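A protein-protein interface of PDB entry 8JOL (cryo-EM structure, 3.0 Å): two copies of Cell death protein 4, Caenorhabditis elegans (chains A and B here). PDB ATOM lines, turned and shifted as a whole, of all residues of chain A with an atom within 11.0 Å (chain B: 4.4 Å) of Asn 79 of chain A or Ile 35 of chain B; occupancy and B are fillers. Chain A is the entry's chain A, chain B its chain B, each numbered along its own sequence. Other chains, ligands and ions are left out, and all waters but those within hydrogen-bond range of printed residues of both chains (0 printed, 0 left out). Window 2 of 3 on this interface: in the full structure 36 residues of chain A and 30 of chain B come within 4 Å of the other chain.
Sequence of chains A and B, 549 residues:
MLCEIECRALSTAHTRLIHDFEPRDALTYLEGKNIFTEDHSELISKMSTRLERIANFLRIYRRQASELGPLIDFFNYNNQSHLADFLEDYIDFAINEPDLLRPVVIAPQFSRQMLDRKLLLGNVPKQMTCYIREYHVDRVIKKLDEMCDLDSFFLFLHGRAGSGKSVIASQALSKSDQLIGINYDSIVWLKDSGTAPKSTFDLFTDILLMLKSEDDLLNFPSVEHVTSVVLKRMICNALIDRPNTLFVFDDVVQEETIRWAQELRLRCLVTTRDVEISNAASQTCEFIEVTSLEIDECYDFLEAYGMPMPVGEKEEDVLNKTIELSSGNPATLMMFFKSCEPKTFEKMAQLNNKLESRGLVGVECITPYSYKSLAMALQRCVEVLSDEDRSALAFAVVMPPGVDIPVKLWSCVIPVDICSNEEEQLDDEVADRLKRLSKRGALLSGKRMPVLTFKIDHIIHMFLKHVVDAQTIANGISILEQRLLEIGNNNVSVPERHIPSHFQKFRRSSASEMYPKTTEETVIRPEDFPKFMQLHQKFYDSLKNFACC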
ATOM      1  N   ASP A  20     -32.789  -4.744   0.386  1.00  0.00           N
ATOM      2  CA  ASP A  20     -31.789  -5.454   1.187  1.00  0.00           C
ATOM      3  C   ASP A  20     -30.512  -5.811   0.406  1.00  0.00           C
ATOM      4  O   ASP A  20     -30.501  -6.749  -0.385  1.00  0.00           O
ATOM      5  CB  ASP A  20     -32.403  -6.722   1.775  1.00  0.00           C
ATOM      6  CG  ASP A  20     -32.862  -7.695   0.709  1.00  0.00           C
ATOM      7  OD1 ASP A  20     -33.353  -7.235  -0.344  1.00  0.00           O
ATOM      8  OD2 ASP A  20     -32.731  -8.921   0.925  1.00  0.00           O
ATOM      9  N   PHE A  21     -29.434  -5.073   0.660  1.00  0.00           N
ATOM     10  CA  PHE A  21     -28.165  -5.238  -0.049  1.00  0.00           C
ATOM     11  C   PHE A  21     -27.213  -4.137   0.405  1.00  0.00           C
ATOM     12  O   PHE A  21     -27.629  -3.159   1.019  1.00  0.00           O
ATOM     13  CB  PHE A  21     -28.381  -5.178  -1.571  1.00  0.00           C
ATOM     14  CG  PHE A  21     -27.105  -5.185  -2.387  1.00  0.00           C
ATOM     15  CD1 PHE A  21     -26.167  -6.200  -2.248  1.00  0.00           C
ATOM     16  CD2 PHE A  21     -26.849  -4.177  -3.302  1.00  0.00           C
ATOM     17  CE1 PHE A  21     -24.991  -6.203  -3.007  1.00  0.00           C
ATOM     18  CE2 PHE A  21     -25.680  -4.176  -4.062  1.00  0.00           C
ATOM     19  CZ  PHE A  21     -24.754  -5.190  -3.911  1.00  0.00           C
ATOM     20  N   GLU A  22     -25.930  -4.294   0.122  1.00  0.00           N
ATOM     21  CA  GLU A  22     -24.966  -3.262   0.452  1.00  0.00           C
ATOM     22  C   GLU A  22     -23.670  -3.519  -0.277  1.00  0.00           C
ATOM     23  O   GLU A  22     -23.074  -4.579  -0.141  1.00  0.00           O
ATOM     24  CB  GLU A  22     -24.706  -3.231   1.940  1.00  0.00           C
ATOM     25  CG  GLU A  22     -23.446  -2.507   2.282  1.00  0.00           C
ATOM     26  CD  GLU A  22     -23.688  -1.067   2.588  1.00  0.00           C
ATOM     27  OE1 GLU A  22     -24.848  -0.715   2.855  1.00  0.00           O
ATOM     28  OE2 GLU A  22     -22.715  -0.292   2.580  1.00  0.00           O
ATOM     29  N   ASP A  25     -20.478  -4.724   1.450  1.00  0.00           N
ATOM     30  CA  ASP A  25     -20.435  -6.148   1.740  1.00  0.00           C
ATOM     31  C   ASP A  25     -19.753  -6.933   0.618  1.00  0.00           C
ATOM     32  O   ASP A  25     -19.156  -7.982   0.866  1.00  0.00           O
ATOM     33  CB  ASP A  25     -21.853  -6.699   1.969  1.00  0.00           C
ATOM     34  CG  ASP A  25     -22.515  -6.151   3.241  1.00  0.00           C
ATOM     35  OD1 ASP A  25     -21.833  -5.502   4.064  1.00  0.00           O
ATOM     36  OD2 ASP A  25     -23.733  -6.385   3.420  1.00  0.00           O
ATOM     37  N   ALA A  26     -19.837  -6.430  -0.610  1.00  0.00           N
ATOM     38  CA  ALA A  26     -19.334  -7.172  -1.766  1.00  0.00           C
ATOM     39  C   ALA A  26     -17.960  -6.715  -2.260  1.00  0.00           C
ATOM     40  O   ALA A  26     -17.312  -7.415  -3.046  1.00  0.00           O
ATOM     41  CB  ALA A  26     -20.350  -7.134  -2.899  1.00  0.00           C
ATOM     42  N   LEU A  71     -21.117 -12.665  -8.624  1.00  0.00           N
ATOM     43  CA  LEU A  71     -22.238 -11.993  -7.987  1.00  0.00           C
ATOM     44  C   LEU A  71     -23.176 -13.031  -7.393  1.00  0.00           C
ATOM     45  O   LEU A  71     -23.453 -13.009  -6.196  1.00  0.00           O
ATOM     46  CB  LEU A  71     -22.976 -11.104  -8.986  1.00  0.00           C
ATOM     47  CG  LEU A  71     -24.073 -10.204  -8.414  1.00  0.00           C
ATOM     48  CD1 LEU A  71     -25.379 -10.955  -8.217  1.00  0.00           C
ATOM     49  CD2 LEU A  71     -23.616  -9.544  -7.121  1.00  0.00           C
ATOM     50  N   ILE A  72     -23.666 -13.946  -8.221  1.00  0.00           N
ATOM     51  CA  ILE A  72     -24.525 -15.004  -7.712  1.00  0.00           C
ATOM     52  C   ILE A  72     -23.842 -15.694  -6.552  1.00  0.00           C
ATOM     53  O   ILE A  72     -24.447 -15.918  -5.505  1.00  0.00           O
ATOM     54  CB  ILE A  72     -24.833 -16.055  -8.786  1.00  0.00           C
ATOM     55  CG1 ILE A  72     -25.572 -15.415  -9.958  1.00  0.00           C
ATOM     56  CG2 ILE A  72     -25.657 -17.183  -8.189  1.00  0.00           C
ATOM     57  CD1 ILE A  72     -26.911 -14.829  -9.576  1.00  0.00           C
ATOM     58  N   ASP A  73     -22.568 -16.018  -6.728  1.00  0.00           N
ATOM     59  CA  ASP A  73     -21.830 -16.701  -5.681  1.00  0.00           C
ATOM     60  C   ASP A  73     -21.884 -15.895  -4.403  1.00  0.00           C
ATOM     61  O   ASP A  73     -21.928 -16.455  -3.308  1.00  0.00           O
ATOM     62  CB  ASP A  73     -20.378 -16.898  -6.104  1.00  0.00           C
ATOM     63  CG  ASP A  73     -20.251 -17.468  -7.502  1.00  0.00           C
ATOM     64  OD1 ASP A  73     -21.270 -17.936  -8.050  1.00  0.00           O
ATOM     65  OD2 ASP A  73     -19.130 -17.449  -8.052  1.00  0.00           O
ATOM     66  N   PHE A  74     -21.883 -14.575  -4.535  1.00  0.00           N
ATOM     67  CA  PHE A  74     -21.871 -13.722  -3.354  1.00  0.00           C
ATOM     68  C   PHE A  74     -23.193 -13.710  -2.596  1.00  0.00           C
ATOM     69  O   PHE A  74     -23.213 -13.994  -1.399  1.00  0.00           O
ATOM     70  CB  PHE A  74     -21.487 -12.289  -3.728  1.00  0.00           C
ATOM     71  CG  PHE A  74     -21.437 -11.360  -2.554  1.00  0.00           C
ATOM     72  CD1 PHE A  74     -20.340 -11.351  -1.711  1.00  0.00           C
ATOM     73  CD2 PHE A  74     -22.492 -10.505  -2.284  1.00  0.00           C
ATOM     74  CE1 PHE A  74     -20.291 -10.502  -0.624  1.00  0.00           C
ATOM     75  CE2 PHE A  74     -22.450  -9.652  -1.200  1.00  0.00           C
ATOM     76  CZ  PHE A  74     -21.347  -9.652  -0.369  1.00  0.00           C
ATOM     77  N   PHE A  75     -24.296 -13.377  -3.264  1.00  0.00           N
ATOM     78  CA  PHE A  75     -25.547 -13.263  -2.517  1.00  0.00           C
ATOM     79  C   PHE A  75     -25.831 -14.576  -1.785  1.00  0.00           C
ATOM     80  O   PHE A  75     -26.495 -14.590  -0.741  1.00  0.00           O
ATOM     81  CB  PHE A  75     -26.719 -12.842  -3.412  1.00  0.00           C
ATOM     82  CG  PHE A  75     -26.717 -11.373  -3.759  1.00  0.00           C
ATOM     83  CD1 PHE A  75     -26.338 -10.427  -2.815  1.00  0.00           C
ATOM     84  CD2 PHE A  75     -27.072 -10.938  -5.028  1.00  0.00           C
ATOM     85  CE1 PHE A  75     -26.323  -9.081  -3.128  1.00  0.00           C
ATOM     86  CE2 PHE A  75     -27.059  -9.592  -5.339  1.00  0.00           C
ATOM     87  CZ  PHE A  75     -26.684  -8.663  -4.386  1.00  0.00           C
ATOM     88  N   ASN A  76     -25.292 -15.670  -2.325  1.00  0.00           N
ATOM     89  CA  ASN A  76     -25.282 -16.951  -1.623  1.00  0.00           C
ATOM     90  C   ASN A  76     -24.575 -16.808  -0.273  1.00  0.00           C
ATOM     91  O   ASN A  76     -25.211 -16.888   0.767  1.00  0.00           O
ATOM     92  CB  ASN A  76     -24.625 -18.052  -2.473  1.00  0.00           C
ATOM     93  CG  ASN A  76     -25.562 -18.615  -3.553  1.00  0.00           C
ATOM     94  OD1 ASN A  76     -26.786 -18.437  -3.498  1.00  0.00           O
ATOM     95  ND2 ASN A  76     -24.981 -19.309  -4.533  1.00  0.00           N
ATOM     96  N   TYR A  77     -23.270 -16.553  -0.288  1.00  0.00           N
ATOM     97  CA  TYR A  77     -22.512 -16.453   0.960  1.00  0.00           C
ATOM     98  C   TYR A  77     -23.025 -15.376   1.935  1.00  0.00           C
ATOM     99  O   TYR A  77     -22.912 -15.544   3.143  1.00  0.00           O
ATOM    100  CB  TYR A  77     -20.983 -16.365   0.702  1.00  0.00           C
ATOM    101  CG  TYR A  77     -20.258 -15.140   1.251  1.00  0.00           C
ATOM    102  CD1 TYR A  77     -20.453 -14.705   2.554  1.00  0.00           C
ATOM    103  CD2 TYR A  77     -19.352 -14.440   0.468  1.00  0.00           C
ATOM    104  CE1 TYR A  77     -19.802 -13.591   3.054  1.00  0.00           C
ATOM    105  CE2 TYR A  77     -18.689 -13.321   0.966  1.00  0.00           C
ATOM    106  CZ  TYR A  77     -18.922 -12.908   2.265  1.00  0.00           C
ATOM    107  OH  TYR A  77     -18.277 -11.808   2.783  1.00  0.00           O
ATOM    108  N   ASN A  78     -23.608 -14.292   1.432  1.00  0.00           N
ATOM    109  CA  ASN A  78     -24.000 -13.172   2.302  1.00  0.00           C
ATOM    110  C   ASN A  78     -25.369 -13.309   2.997  1.00  0.00           C
ATOM    111  O   ASN A  78     -25.915 -12.318   3.482  1.00  0.00           O
ATOM    112  CB  ASN A  78     -23.935 -11.845   1.530  1.00  0.00           C
ATOM    113  CG  ASN A  78     -23.185 -10.756   2.284  1.00  0.00           C
ATOM    114  OD1 ASN A  78     -22.423 -11.032   3.211  1.00  0.00           O
ATOM    115  ND2 ASN A  78     -23.391  -9.507   1.875  1.00  0.00           N
ATOM    116  N   ASN A  79     -25.914 -14.524   3.046  1.00  0.00           N
ATOM    117  CA  ASN A  79     -27.235 -14.768   3.647  1.00  0.00           C
ATOM    118  C   ASN A  79     -28.360 -14.037   2.906  1.00  0.00           C
ATOM    119  O   ASN A  79     -29.510 -13.991   3.367  1.00  0.00           O
ATOM    120  CB  ASN A  79     -27.247 -14.416   5.143  1.00  0.00           C
ATOM    121  CG  ASN A  79     -27.331 -15.646   6.048  1.00  0.00           C
ATOM    122  OD1 ASN A  79     -27.782 -16.712   5.631  1.00  0.00           O
ATOM    123  ND2 ASN A  79     -26.901 -15.491   7.297  1.00  0.00           N
ATOM    124  N   GLN A  80     -28.003 -13.459   1.762  1.00  0.00           N
ATOM    125  CA  GLN A  80     -28.957 -12.834   0.854  1.00  0.00           C
ATOM    126  C   GLN A  80     -29.218 -13.771  -0.327  1.00  0.00           C
ATOM    127  O   GLN A  80     -29.311 -13.331  -1.468  1.00  0.00           O
ATOM    128  CB  GLN A  80     -28.436 -11.465   0.370  1.00  0.00           C
ATOM    129  CG  GLN A  80     -28.612 -10.307   1.375  1.00  0.00           C
ATOM    130  CD  GLN A  80     -27.672  -9.121   1.121  1.00  0.00           C
ATOM    131  OE1 GLN A  80     -26.677  -9.239   0.405  1.00  0.00           O
ATOM    132  NE2 GLN A  80     -27.982  -7.977   1.725  1.00  0.00           N
ATOM    133  N   SER A  81     -29.335 -15.066  -0.047  1.00  0.00           N
ATOM    134  CA  SER A  81     -29.515 -16.052  -1.103  1.00  0.00           C
ATOM    135  C   SER A  81     -30.841 -15.950  -1.813  1.00  0.00           C
ATOM    136  O   SER A  81     -30.968 -16.434  -2.929  1.00  0.00           O
ATOM    137  CB  SER A  81     -29.334 -17.456  -0.579  1.00  0.00           C
ATOM    138  OG  SER A  81     -27.968 -17.679  -0.352  1.00  0.00           O
ATOM    139  N   HIS A  82     -31.826 -15.318  -1.185  1.00  0.00           N
ATOM    140  CA  HIS A  82     -33.096 -15.075  -1.863  1.00  0.00           C
ATOM    141  C   HIS A  82     -32.887 -14.168  -3.060  1.00  0.00           C
ATOM    142  O   HIS A  82     -33.767 -14.047  -3.908  1.00  0.00           O
ATOM    143  CB  HIS A  82     -34.123 -14.470  -0.914  1.00  0.00           C
ATOM    144  CG  HIS A  82     -33.557 -13.436   0.004  1.00  0.00           C
ATOM    145  ND1 HIS A  82     -32.997 -13.754   1.226  1.00  0.00           N
ATOM    146  CD2 HIS A  82     -33.466 -12.093  -0.116  1.00  0.00           C
ATOM    147  CE1 HIS A  82     -32.583 -12.645   1.815  1.00  0.00           C
ATOM    148  NE2 HIS A  82     -32.856 -11.623   1.023  1.00  0.00           N
ATOM    149  N   LEU A  83     -31.715 -13.534  -3.113  1.00  0.00           N
ATOM    150  CA  LEU A  83     -31.299 -12.721  -4.260  1.00  0.00           C
ATOM    151  C   LEU A  83     -30.568 -13.537  -5.339  1.00  0.00           C
ATOM    152  O   LEU A  83     -31.033 -13.614  -6.474  1.00  0.00           O
ATOM    153  CB  LEU A  83     -30.432 -11.532  -3.817  1.00  0.00           C
ATOM    154  CG  LEU A  83     -31.071 -10.423  -2.974  1.00  0.00           C
ATOM    155  CD1 LEU A  83     -30.060  -9.334  -2.679  1.00  0.00           C
ATOM    156  CD2 LEU A  83     -32.291  -9.832  -3.655  1.00  0.00           C
ATOM    157  N   ALA A  84     -29.437 -14.151  -4.992  1.00  0.00           N
ATOM    158  CA  ALA A  84     -28.661 -14.929  -5.966  1.00  0.00           C
ATOM    159  C   ALA A  84     -29.479 -16.052  -6.598  1.00  0.00           C
ATOM    160  O   ALA A  84     -29.143 -16.541  -7.674  1.00  0.00           O
ATOM    161  CB  ALA A  84     -27.396 -15.480  -5.338  1.00  0.00           C
ATOM    162  N   ASP A  85     -30.555 -16.453  -5.928  1.00  0.00           N
ATOM    163  CA  ASP A  85     -31.470 -17.455  -6.471  1.00  0.00           C
ATOM    164  C   ASP A  85     -32.367 -16.858  -7.569  1.00  0.00           C
ATOM    165  O   ASP A  85     -32.538 -17.458  -8.629  1.00  0.00           O
ATOM    166  CB  ASP A  85     -32.308 -18.105  -5.355  1.00  0.00           C
ATOM    167  CG  ASP A  85     -31.451 -18.816  -4.299  1.00  0.00           C
ATOM    168  OD1 ASP A  85     -30.236 -19.021  -4.527  1.00  0.00           O
ATOM    169  OD2 ASP A  85     -31.998 -19.170  -3.230  1.00  0.00           O
ATOM    170  N   TYR B  29     -25.638 -16.198  18.283  1.00  0.00           N
ATOM    171  CA  TYR B  29     -26.962 -16.772  18.065  1.00  0.00           C
ATOM    172  C   TYR B  29     -27.502 -16.474  16.665  1.00  0.00           C
ATOM    173  O   TYR B  29     -28.411 -17.159  16.191  1.00  0.00           O
ATOM    174  CB  TYR B  29     -27.950 -16.301  19.139  1.00  0.00           C
ATOM    175  CG  TYR B  29     -29.363 -16.815  18.940  1.00  0.00           C
ATOM    176  CD1 TYR B  29     -29.695 -18.129  19.240  1.00  0.00           C
ATOM    177  CD2 TYR B  29     -30.359 -15.986  18.455  1.00  0.00           C
ATOM    178  CE1 TYR B  29     -30.985 -18.601  19.057  1.00  0.00           C
ATOM    179  CE2 TYR B  29     -31.646 -16.445  18.268  1.00  0.00           C
ATOM    180  CZ  TYR B  29     -31.956 -17.753  18.569  1.00  0.00           C
ATOM    181  OH  TYR B  29     -33.245 -18.209  18.382  1.00  0.00           O
ATOM    182  N   LEU B  30     -26.961 -15.453  16.016  1.00  0.00           N
ATOM    183  CA  LEU B  30     -27.406 -15.131  14.669  1.00  0.00           C
ATOM    184  C   LEU B  30     -26.539 -15.865  13.663  1.00  0.00           C
ATOM    185  O   LEU B  30     -27.054 -16.524  12.763  1.00  0.00           O
ATOM    186  CB  LEU B  30     -27.384 -13.621  14.432  1.00  0.00           C
ATOM    187  CG  LEU B  30     -28.308 -12.845  15.374  1.00  0.00           C
ATOM    188  CD1 LEU B  30     -28.766 -11.547  14.733  1.00  0.00           C
ATOM    189  CD2 LEU B  30     -29.516 -13.685  15.759  1.00  0.00           C
ATOM    190  N   GLU B  31     -25.225 -15.779  13.825  1.00  0.00           N
ATOM    191  CA  GLU B  31     -24.335 -16.515  12.944  1.00  0.00           C
ATOM    192  C   GLU B  31     -24.674 -17.988  13.045  1.00  0.00           C
ATOM    193  O   GLU B  31     -24.720 -18.691  12.037  1.00  0.00           O
ATOM    194  CB  GLU B  31     -22.879 -16.287  13.333  1.00  0.00           C
ATOM    195  CG  GLU B  31     -22.458 -14.828  13.331  1.00  0.00           C
ATOM    196  CD  GLU B  31     -21.124 -14.617  14.014  1.00  0.00           C
ATOM    197  OE1 GLU B  31     -20.092 -15.039  13.451  1.00  0.00           O
ATOM    198  OE2 GLU B  31     -21.106 -14.027  15.115  1.00  0.00           O
ATOM    199  N   LYS B  33     -27.493 -19.231  13.707  1.00  0.00           N
ATOM    200  CA  LYS B  33     -28.744 -19.438  12.989  1.00  0.00           C
ATOM    201  C   LYS B  33     -28.621 -18.950  11.559  1.00  0.00           C
ATOM    202  O   LYS B  33     -29.626 -18.687  10.899  1.00  0.00           O
ATOM    203  CB  LYS B  33     -29.893 -18.717  13.687  1.00  0.00           C
ATOM    204  CG  LYS B  33     -30.266 -19.316  15.028  1.00  0.00           C
ATOM    205  CD  LYS B  33     -31.465 -18.604  15.624  1.00  0.00           C
ATOM    206  CE  LYS B  33     -32.696 -18.745  14.745  1.00  0.00           C
ATOM    207  NZ  LYS B  33     -33.904 -18.186  15.410  1.00  0.00           N
ATOM    208  N   ASN B  34     -27.388 -18.818  11.081  1.00  0.00           N
ATOM    209  CA  ASN B  34     -27.167 -18.363   9.716  1.00  0.00           C
ATOM    210  C   ASN B  34     -27.884 -17.050   9.488  1.00  0.00           C
ATOM    211  O   ASN B  34     -28.674 -16.921   8.553  1.00  0.00           O
ATOM    212  CB  ASN B  34     -27.646 -19.413   8.714  1.00  0.00           C
ATOM    213  CG  ASN B  34     -26.927 -20.739   8.872  1.00  0.00           C
ATOM    214  OD1 ASN B  34     -27.331 -21.747   8.295  1.00  0.00           O
ATOM    215  ND2 ASN B  34     -25.856 -20.745   9.658  1.00  0.00           N
ATOM    216  N   ILE B  35     -27.628 -16.075  10.350  1.00  0.00           N
ATOM    217  CA  ILE B  35     -28.249 -14.768  10.207  1.00  0.00           C
ATOM    218  C   ILE B  35     -27.174 -13.713  10.015  1.00  0.00           C
ATOM    219  O   ILE B  35     -27.443 -12.626   9.504  1.00  0.00           O
ATOM    220  CB  ILE B  35     -29.097 -14.419  11.439  1.00  0.00           C
ATOM    221  CG1 ILE B  35     -30.046 -15.573  11.765  1.00  0.00           C
ATOM    222  CG2 ILE B  35     -29.874 -13.130  11.215  1.00  0.00           C
ATOM    223  CD1 ILE B  35     -30.837 -15.369  13.035  1.00  0.00           C
ATOM    224  N   PHE B  36     -25.948 -14.036  10.413  1.00  0.00           N
ATOM    225  CA  PHE B  36     -24.857 -13.072  10.300  1.00  0.00           C
ATOM    226  C   PHE B  36     -23.624 -13.636   9.609  1.00  0.00           C
ATOM    227  O   PHE B  36     -23.169 -14.732   9.933  1.00  0.00           O
ATOM    228  CB  PHE B  36     -24.487 -12.528  11.682  1.00  0.00           C
ATOM    229  CG  PHE B  36     -25.173 -11.240  12.018  1.00  0.00           C
ATOM    230  CD1 PHE B  36     -26.551 -11.178  12.112  1.00  0.00           C
ATOM    231  CD2 PHE B  36     -24.440 -10.085  12.215  1.00  0.00           C
ATOM    232  CE1 PHE B  36     -27.187  -9.989  12.412  1.00  0.00           C
ATOM    233  CE2 PHE B  36     -25.069  -8.895  12.517  1.00  0.00           C
ATOM    234  CZ  PHE B  36     -26.444  -8.845  12.619  1.00  0.00           C
ATOM    235  N   THR B  37     -23.081 -12.883   8.660  1.00  0.00           N
ATOM    236  CA  THR B  37     -21.894 -13.321   7.928  1.00  0.00           C
ATOM    237  C   THR B  37     -20.658 -12.947   8.738  1.00  0.00           C
ATOM    238  O   THR B  37     -20.693 -11.990   9.514  1.00  0.00           O
ATOM    239  CB  THR B  37     -21.797 -12.650   6.542  1.00  0.00           C
ATOM    240  OG1 THR B  37     -21.450 -11.270   6.700  1.00  0.00           O
ATOM    241  CG2 THR B  37     -23.115 -12.759   5.783  1.00  0.00           C
ATOM    242  N   GLN B  64     -31.373  -8.347   6.548  1.00  0.00           N
ATOM    243  CA  GLN B  64     -31.010  -9.763   6.456  1.00  0.00           C
ATOM    244  C   GLN B  64     -32.117 -10.795   6.710  1.00  0.00           C
ATOM    245  O   GLN B  64     -32.179 -11.825   6.029  1.00  0.00           O
ATOM    246  CB  GLN B  64     -29.837 -10.032   7.395  1.00  0.00           C
ATOM    247  CG  GLN B  64     -28.542  -9.379   6.955  1.00  0.00           C
ATOM    248  CD  GLN B  64     -27.857 -10.157   5.851  1.00  0.00           C
ATOM    249  OE1 GLN B  64     -26.643 -10.338   5.869  1.00  0.00           O
ATOM    250  NE2 GLN B  64     -28.637 -10.637   4.890  1.00  0.00           N
ATOM    251  N   PRO B  70     -36.640 -14.414  15.060  1.00  0.00           N
ATOM    252  CA  PRO B  70     -35.370 -14.718  15.737  1.00  0.00           C
ATOM    253  C   PRO B  70     -34.966 -13.679  16.776  1.00  0.00           C
ATOM    254  O   PRO B  70     -34.343 -14.032  17.777  1.00  0.00           O
ATOM    255  CB  PRO B  70     -34.356 -14.713  14.589  1.00  0.00           C
ATOM    256  CG  PRO B  70     -35.158 -15.039  13.377  1.00  0.00           C
ATOM    257  CD  PRO B  70     -36.491 -14.388  13.595  1.00  0.00           C
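The side-chain amide oxygen (OE1) of Gln 64 of chain B sits close to the backbone carbonyl oxygen (O) of Asn 78 of chain A (3.2 Å). The side-chain amide nitrogen (ND2) of Asn 79 of chain A sits at hydrogen-bond distance from the backbone carbonyl oxygen (O) of Asn 34 of chain B (2.6 Å). The backbone NH of Ile 35 of chain B sits close to the side-chain amide nitrogen of Asn 79 of chain A (3.2 Å).
The backbone carbonyl oxygen of Phe 75 of chain A lies close to the backbone NH of Gln 80 of chain A (3.1 Å). N of Phe 21 of chain A sits close to NE2 of Gln 80 of chain A. ND2 of Asn 34 of chain B sits at hydrogen-bond distance from O of Glu 31 of chain B. ND2 of Asn 78 of chain A sits close to OD2 of Asp 25 of chain A. O of Leu 30 of chain B is in hydrogen-bond range of N of Ile 35 of chain B (2.5 Å).
Among the printed residues, pairs that only touch across the chains: Tyr 77 of chain A with Thr 37 of chain B (3.8 Å), Asn 78 of chain A with Thr 37 of chain B (3.2 Å), Asn 79 of chain A with Phe 36 of chain B (3.6 Å), Asn 79 of chain A with Gln 64 of chain B (3.8 Å) and Gln 80 of chain A with Gln 64 of chain B (3.5 Å).
Asn 79 of chain A touches just these residues of chain B: Asn 34, Ile 35, Phe 36 and Gln 64. Ile 35 of chain B touches one residue of chain A. No residue of chain A comes within 4 Å of Lys 33 of chain B. Of chain A, only Asn 79 comes within 4 Å of Asn 34 of chain B. Phe 36 of chain B touches just one residue of chain A: Asn 79. Of chain A, only Tyr 77 and Asn 78 come within 4 Å of Thr 37 of chain B. Gln 64 of chain B touches three residues of chain A. Printed residues of chain B within 4 Å of Asn 78 of chain A: Thr 37 and Gln 64. Printed residues of chain B within 4 Å of Gln 80 of chain A: Gln 64. Of the printed residues of chain B, Tyr 77 of chain A touches Thr 37 (3.8 Å). Ile 72 of chain A touches none of the printed residues of chain B. The nearest residue of chain B that does not touch Asn 79 of chain A is Thr 37 of chain B (4.3 Å). The nearest printed residue of chain B that does not touch Gln 80 of chain A is Thr 37 of chain B (6.4 Å).
Printed residues of chain B that touch a printed residue of chain A: Asn 34, Ile 35, Phe 36, Thr 37 and Gln 64. Among the printed residues, 8 pairs touch across the chains.
No position is printed for both chains. Of the 8 pairs that touch across the chains among the printed residues, none has its exchanged pair printed and touching as well.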
